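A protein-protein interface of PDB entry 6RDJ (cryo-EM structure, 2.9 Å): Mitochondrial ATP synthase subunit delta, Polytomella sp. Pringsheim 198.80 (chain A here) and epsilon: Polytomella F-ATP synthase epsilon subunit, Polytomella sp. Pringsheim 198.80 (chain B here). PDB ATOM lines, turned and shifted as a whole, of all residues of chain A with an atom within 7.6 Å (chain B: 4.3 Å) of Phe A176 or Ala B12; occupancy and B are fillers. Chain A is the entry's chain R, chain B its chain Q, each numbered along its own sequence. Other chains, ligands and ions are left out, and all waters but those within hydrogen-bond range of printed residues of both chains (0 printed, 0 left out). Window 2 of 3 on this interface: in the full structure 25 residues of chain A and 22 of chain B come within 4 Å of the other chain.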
ATOM      1  N   PRO A 172     -16.665  16.302  19.394  1.00  0.00           N
ATOM      2  CA  PRO A 172     -17.659  15.244  19.615  1.00  0.00           C
ATOM      3  C   PRO A 172     -18.285  15.322  20.999  1.00  0.00           C
ATOM      4  O   PRO A 172     -18.038  16.272  21.748  1.00  0.00           O
ATOM      5  CB  PRO A 172     -16.841  13.960  19.440  1.00  0.00           C
ATOM      6  CG  PRO A 172     -15.473  14.346  19.866  1.00  0.00           C
ATOM      7  CD  PRO A 172     -15.290  15.778  19.440  1.00  0.00           C
ATOM      8  N   THR A 173     -19.087  14.320  21.354  1.00  0.00           N
ATOM      9  CA  THR A 173     -19.714  14.259  22.671  1.00  0.00           C
ATOM     10  C   THR A 173     -18.760  13.790  23.765  1.00  0.00           C
ATOM     11  O   THR A 173     -19.173  13.710  24.929  1.00  0.00           O
ATOM     12  CB  THR A 173     -20.941  13.343  22.630  1.00  0.00           C
ATOM     13  OG1 THR A 173     -20.525  11.989  22.405  1.00  0.00           O
ATOM     14  CG2 THR A 173     -21.891  13.774  21.526  1.00  0.00           C
ATOM     15  N   ASP A 174     -17.516  13.467  23.422  1.00  0.00           N
ATOM     16  CA  ASP A 174     -16.503  13.159  24.420  1.00  0.00           C
ATOM     17  C   ASP A 174     -16.196  14.394  25.252  1.00  0.00           C
ATOM     18  O   ASP A 174     -16.060  15.493  24.722  1.00  0.00           O
ATOM     19  CB  ASP A 174     -15.230  12.670  23.736  1.00  0.00           C
ATOM     20  CG  ASP A 174     -14.349  11.847  24.649  1.00  0.00           C
ATOM     21  OD1 ASP A 174     -14.626  11.788  25.865  1.00  0.00           O
ATOM     22  OD2 ASP A 174     -13.364  11.267  24.149  1.00  0.00           O
ATOM     23  N   GLU A 175     -16.074  14.209  26.560  1.00  0.00           N
ATOM     24  CA  GLU A 175     -15.609  15.285  27.422  1.00  0.00           C
ATOM     25  C   GLU A 175     -14.092  15.375  27.424  1.00  0.00           C
ATOM     26  O   GLU A 175     -13.531  16.461  27.635  1.00  0.00           O
ATOM     27  CB  GLU A 175     -16.136  15.077  28.846  1.00  0.00           C
ATOM     28  CG  GLU A 175     -15.692  13.775  29.501  1.00  0.00           C
ATOM     29  CD  GLU A 175     -16.280  13.578  30.882  1.00  0.00           C
ATOM     30  OE1 GLU A 175     -17.049  14.457  31.331  1.00  0.00           O
ATOM     31  OE2 GLU A 175     -15.975  12.548  31.520  1.00  0.00           O
ATOM     32  N   PHE A 176     -13.436  14.252  27.137  1.00  0.00           N
ATOM     33  CA  PHE A 176     -11.984  14.193  27.100  1.00  0.00           C
ATOM     34  C   PHE A 176     -11.450  15.008  25.930  1.00  0.00           C
ATOM     35  O   PHE A 176     -10.504  15.790  26.077  1.00  0.00           O
ATOM     36  CB  PHE A 176     -11.559  12.738  26.975  1.00  0.00           C
ATOM     37  CG  PHE A 176     -10.205  12.454  27.507  1.00  0.00           C
ATOM     38  CD1 PHE A 176     -10.049  12.115  28.840  1.00  0.00           C
ATOM     39  CD2 PHE A 176      -9.085  12.551  26.706  1.00  0.00           C
ATOM     40  CE1 PHE A 176      -8.812  11.836  29.353  1.00  0.00           C
ATOM     41  CE2 PHE A 176      -7.838  12.283  27.219  1.00  0.00           C
ATOM     42  CZ  PHE A 176      -7.709  11.926  28.542  1.00  0.00           C
ATOM     43  N   GLU A 177     -12.072  14.858  24.758  1.00  0.00           N
ATOM     44  CA  GLU A 177     -11.667  15.659  23.616  1.00  0.00           C
ATOM     45  C   GLU A 177     -12.115  17.102  23.745  1.00  0.00           C
ATOM     46  O   GLU A 177     -11.471  17.969  23.158  1.00  0.00           O
ATOM     47  CB  GLU A 177     -12.194  15.071  22.308  1.00  0.00           C
ATOM     48  CG  GLU A 177     -11.289  15.361  21.102  1.00  0.00           C
ATOM     49  CD  GLU A 177     -11.645  16.645  20.348  1.00  0.00           C
ATOM     50  OE1 GLU A 177     -12.678  17.276  20.654  1.00  0.00           O
ATOM     51  OE2 GLU A 177     -10.877  17.033  19.444  1.00  0.00           O
ATOM     52  N   GLN A 178     -13.176  17.393  24.508  1.00  0.00           N
ATOM     53  CA  GLN A 178     -13.473  18.789  24.824  1.00  0.00           C
ATOM     54  C   GLN A 178     -12.354  19.421  25.630  1.00  0.00           C
ATOM     55  O   GLN A 178     -11.950  20.555  25.353  1.00  0.00           O
ATOM     56  CB  GLN A 178     -14.792  18.932  25.586  1.00  0.00           C
ATOM     57  CG  GLN A 178     -16.049  18.674  24.790  1.00  0.00           C
ATOM     58  CD  GLN A 178     -16.325  19.726  23.739  1.00  0.00           C
ATOM     59  OE1 GLN A 178     -16.912  19.431  22.698  1.00  0.00           O
ATOM     60  NE2 GLN A 178     -15.922  20.962  24.009  1.00  0.00           N
ATOM     61  N   ALA A 179     -11.814  18.684  26.603  1.00  0.00           N
ATOM     62  CA  ALA A 179     -10.704  19.214  27.386  1.00  0.00           C
ATOM     63  C   ALA A 179      -9.446  19.373  26.538  1.00  0.00           C
ATOM     64  O   ALA A 179      -8.784  20.419  26.590  1.00  0.00           O
ATOM     65  CB  ALA A 179     -10.445  18.310  28.585  1.00  0.00           C
ATOM     66  N   ALA A 180      -9.124  18.361  25.725  1.00  0.00           N
ATOM     67  CA  ALA A 180      -7.939  18.422  24.872  1.00  0.00           C
ATOM     68  C   ALA A 180      -8.071  19.485  23.792  1.00  0.00           C
ATOM     69  O   ALA A 180      -7.094  20.171  23.472  1.00  0.00           O
ATOM     70  CB  ALA A 180      -7.678  17.061  24.237  1.00  0.00           C
ATOM     71  N   ASN A 181      -9.278  19.683  23.272  1.00  0.00           N
ATOM     72  CA  ASN A 181      -9.516  20.691  22.254  1.00  0.00           C
ATOM     73  C   ASN A 181      -9.522  22.096  22.849  1.00  0.00           C
ATOM     74  O   ASN A 181      -9.090  23.048  22.193  1.00  0.00           O
ATOM     75  CB  ASN A 181     -10.834  20.375  21.555  1.00  0.00           C
ATOM     76  CG  ASN A 181     -11.137  21.319  20.438  1.00  0.00           C
ATOM     77  OD1 ASN A 181     -12.231  21.871  20.356  1.00  0.00           O
ATOM     78  ND2 ASN A 181     -10.165  21.524  19.563  1.00  0.00           N
ATOM     79  N   ARG A 182      -9.982  22.244  24.097  1.00  0.00           N
ATOM     80  CA  ARG A 182      -9.901  23.539  24.764  1.00  0.00           C
ATOM     81  C   ARG A 182      -8.457  23.909  25.063  1.00  0.00           C
ATOM     82  O   ARG A 182      -8.054  25.067  24.881  1.00  0.00           O
ATOM     83  CB  ARG A 182     -10.724  23.530  26.051  1.00  0.00           C
ATOM     84  CG  ARG A 182     -10.644  24.829  26.833  1.00  0.00           C
ATOM     85  CD  ARG A 182     -11.566  24.830  28.025  1.00  0.00           C
ATOM     86  NE  ARG A 182     -11.288  25.958  28.905  1.00  0.00           N
ATOM     87  CZ  ARG A 182     -11.962  26.216  30.018  1.00  0.00           C
ATOM     88  NH1 ARG A 182     -12.956  25.426  30.385  1.00  0.00           N
ATOM     89  NH2 ARG A 182     -11.639  27.260  30.763  1.00  0.00           N
ATOM     90  N   PHE B   8     -10.725  22.271  34.286  1.00  0.00           N
ATOM     91  CA  PHE B   8     -11.502  21.647  33.217  1.00  0.00           C
ATOM     92  C   PHE B   8     -10.911  20.321  32.762  1.00  0.00           C
ATOM     93  O   PHE B   8     -11.641  19.467  32.252  1.00  0.00           O
ATOM     94  CB  PHE B   8     -11.641  22.604  32.032  1.00  0.00           C
ATOM     95  CG  PHE B   8     -10.359  22.884  31.302  1.00  0.00           C
ATOM     96  CD1 PHE B   8     -10.040  22.200  30.141  1.00  0.00           C
ATOM     97  CD2 PHE B   8      -9.499  23.868  31.745  1.00  0.00           C
ATOM     98  CE1 PHE B   8      -8.873  22.463  29.468  1.00  0.00           C
ATOM     99  CE2 PHE B   8      -8.332  24.138  31.072  1.00  0.00           C
ATOM    100  CZ  PHE B   8      -8.023  23.436  29.930  1.00  0.00           C
ATOM    101  N   TYR B   9      -9.606  20.130  32.926  1.00  0.00           N
ATOM    102  CA  TYR B   9      -9.042  18.813  32.674  1.00  0.00           C
ATOM    103  C   TYR B   9      -9.430  17.834  33.768  1.00  0.00           C
ATOM    104  O   TYR B   9      -9.653  16.654  33.490  1.00  0.00           O
ATOM    105  CB  TYR B   9      -7.523  18.898  32.539  1.00  0.00           C
ATOM    106  CG  TYR B   9      -6.830  19.744  33.576  1.00  0.00           C
ATOM    107  CD1 TYR B   9      -6.535  21.072  33.326  1.00  0.00           C
ATOM    108  CD2 TYR B   9      -6.441  19.204  34.790  1.00  0.00           C
ATOM    109  CE1 TYR B   9      -5.898  21.841  34.261  1.00  0.00           C
ATOM    110  CE2 TYR B   9      -5.803  19.968  35.730  1.00  0.00           C
ATOM    111  CZ  TYR B   9      -5.534  21.283  35.459  1.00  0.00           C
ATOM    112  OH  TYR B   9      -4.896  22.052  36.395  1.00  0.00           O
ATOM    113  N   ARG B  10      -9.543  18.304  35.007  1.00  0.00           N
ATOM    114  CA  ARG B  10      -9.896  17.423  36.108  1.00  0.00           C
ATOM    115  C   ARG B  10     -11.360  17.019  36.055  1.00  0.00           C
ATOM    116  O   ARG B  10     -11.704  15.904  36.456  1.00  0.00           O
ATOM    117  CB  ARG B  10      -9.579  18.107  37.433  1.00  0.00           C
ATOM    118  CG  ARG B  10      -9.589  17.197  38.621  1.00  0.00           C
ATOM    119  CD  ARG B  10      -8.447  16.213  38.548  1.00  0.00           C
ATOM    120  NE  ARG B  10      -7.149  16.874  38.562  1.00  0.00           N
ATOM    121  CZ  ARG B  10      -6.001  16.236  38.753  1.00  0.00           C
ATOM    122  NH1 ARG B  10      -5.999  14.928  38.950  1.00  0.00           N
ATOM    123  NH2 ARG B  10      -4.862  16.902  38.757  1.00  0.00           N
ATOM    124  N   VAL B  11     -12.230  17.905  35.564  1.00  0.00           N
ATOM    125  CA  VAL B  11     -13.640  17.564  35.404  1.00  0.00           C
ATOM    126  C   VAL B  11     -13.819  16.514  34.322  1.00  0.00           C
ATOM    127  O   VAL B  11     -14.636  15.597  34.464  1.00  0.00           O
ATOM    128  CB  VAL B  11     -14.470  18.826  35.108  1.00  0.00           C
ATOM    129  CG1 VAL B  11     -15.950  18.512  35.136  1.00  0.00           C
ATOM    130  CG2 VAL B  11     -14.188  19.884  36.138  1.00  0.00           C
ATOM    131  N   ALA B  12     -13.036  16.589  33.252  1.00  0.00           N
ATOM    132  CA  ALA B  12     -13.134  15.627  32.165  1.00  0.00           C
ATOM    133  C   ALA B  12     -12.380  14.333  32.432  1.00  0.00           C
ATOM    134  O   ALA B  12     -12.098  13.599  31.482  1.00  0.00           O
ATOM    135  CB  ALA B  12     -12.629  16.253  30.866  1.00  0.00           C
ATOM    136  N   GLY B  13     -12.028  14.040  33.685  1.00  0.00           N
ATOM    137  CA  GLY B  13     -11.328  12.824  34.035  1.00  0.00           C
ATOM    138  C   GLY B  13      -9.848  12.825  33.743  1.00  0.00           C
ATOM    139  O   GLY B  13      -9.155  11.886  34.149  1.00  0.00           O
ATOM    140  N   MET B  14      -9.338  13.841  33.063  1.00  0.00           N
ATOM    141  CA  MET B  14      -7.944  13.883  32.670  1.00  0.00           C
ATOM    142  C   MET B  14      -7.078  14.285  33.854  1.00  0.00           C
ATOM    143  O   MET B  14      -7.466  15.122  34.669  1.00  0.00           O
ATOM    144  CB  MET B  14      -7.769  14.870  31.517  1.00  0.00           C
ATOM    145  CG  MET B  14      -6.465  14.787  30.794  1.00  0.00           C
ATOM    146  SD  MET B  14      -6.391  16.029  29.507  1.00  0.00           S
ATOM    147  CE  MET B  14      -7.878  15.649  28.622  1.00  0.00           C
ATOM    148  N   ARG B  18      -1.378  14.350  32.030  1.00  0.00           N
ATOM    149  CA  ARG B  18      -1.792  14.112  30.659  1.00  0.00           C
ATOM    150  C   ARG B  18      -2.188  15.405  29.975  1.00  0.00           C
ATOM    151  O   ARG B  18      -1.904  15.591  28.792  1.00  0.00           O
ATOM    152  CB  ARG B  18      -2.940  13.120  30.607  1.00  0.00           C
ATOM    153  CG  ARG B  18      -3.140  12.586  29.218  1.00  0.00           C
ATOM    154  CD  ARG B  18      -4.281  11.631  29.165  1.00  0.00           C
ATOM    155  NE  ARG B  18      -4.025  10.388  29.866  1.00  0.00           N
ATOM    156  CZ  ARG B  18      -3.492   9.323  29.289  1.00  0.00           C
ATOM    157  NH1 ARG B  18      -3.164   9.365  28.008  1.00  0.00           N
ATOM    158  NH2 ARG B  18      -3.292   8.217  29.989  1.00  0.00           N
ATOM    159  N   LYS B  71      -4.103  11.747  23.056  1.00  0.00           N
ATOM    160  CA  LYS B  71      -5.058  12.841  23.181  1.00  0.00           C
ATOM    161  C   LYS B  71      -6.440  12.339  23.567  1.00  0.00           C
ATOM    162  O   LYS B  71      -7.204  13.064  24.212  1.00  0.00           O
ATOM    163  CB  LYS B  71      -5.158  13.623  21.875  1.00  0.00           C
ATOM    164  CG  LYS B  71      -3.884  14.288  21.393  1.00  0.00           C
ATOM    165  CD  LYS B  71      -4.005  14.577  19.902  1.00  0.00           C
ATOM    166  CE  LYS B  71      -3.075  15.679  19.438  1.00  0.00           C
ATOM    167  NZ  LYS B  71      -1.646  15.401  19.734  1.00  0.00           N
ATOM    168  N   THR B  72      -6.789  11.127  23.153  1.00  0.00           N
ATOM    169  CA  THR B  72      -8.097  10.562  23.428  1.00  0.00           C
ATOM    170  C   THR B  72      -8.048   9.836  24.778  1.00  0.00           C
ATOM    171  O   THR B  72      -6.981   9.651  25.365  1.00  0.00           O
ATOM    172  CB  THR B  72      -8.500   9.641  22.275  1.00  0.00           C
ATOM    173  OG1 THR B  72      -8.050  10.228  21.049  1.00  0.00           O
ATOM    174  CG2 THR B  72     -10.014   9.538  22.137  1.00  0.00           C
ATOM    175  N   ALA B  73      -9.218   9.438  25.277  1.00  0.00           N
ATOM    176  CA  ALA B  73      -9.376   8.923  26.630  1.00  0.00           C
ATOM    177  C   ALA B  73      -8.706   7.566  26.814  1.00  0.00           C
ATOM    178  O   ALA B  73      -8.339   6.883  25.857  1.00  0.00           O
ATOM    179  CB  ALA B  73     -10.857   8.802  26.980  1.00  0.00           C
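Ala B12 touches Phe A176 (O to CD1, 3.7 Å).
Met B14 touches Phe A176.
Arg B18 touches Phe A176 (CD to CZ, 3.5 Å).
Phe A176 touches Lys B71.
Phe A176 touches Thr B72.
Phe A176 touches Ala B73.
Phe B8 touches Ala A179 (CE1 to O, 3.5 Å).
Ala B12 touches Ala A179 (CB to CB, 3.8 Å).
CB of Ala A179 touches CE of Met B14 (3.7 Å).
NH1 of Arg A182 touches CB of Phe B8, at 3.5 Å.
Of the 11 printed residues of chain B, 7 touch a printed residue of chain A.
Hydrophobic or aromatic side chains of chain B that line the printed part of chain A: Phe B8, Ala B12, Met B14 and Ala B73.
Among the printed residues, 11 pairs touch across the chains.
Among the printed residues, no Asp or Glu carboxylate lies within 4 Å of a Lys or Arg side-chain nitrogen of the other chain.
Asp A174 touches none of the printed residues of chain B.
Phe A176 touches just these residues of chain B: Ala B12, Met B14, Arg B18, Lys B71, Thr B72 and Ala B73.
Printed residues of chain A within 4 Å of Phe B8: Ala A179 (3.5 Å) and Arg A182 (3.5 Å).
Printed residues of chain A within 4 Å of Lys B71: Phe A176.
Of the printed residues of chain A, Thr B72 touches Phe A176.
Printed residues of chain A within 4 Å of Ala B73: Phe A176 (3.4 Å).
The nearest printed residue of chain B that does not touch Phe A176 is Gly B13 (4.6 Å).
The nearest printed residue of chain B that does not touch Glu A175 is Val B11 (4.1 Å).
N of Phe A176 lies within hydrogen-bond range of OD1 of Asp A174, at 3.0 Å.
O of Tyr B9 is in hydrogen-bond range of N of Met B14 (2.9 Å).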
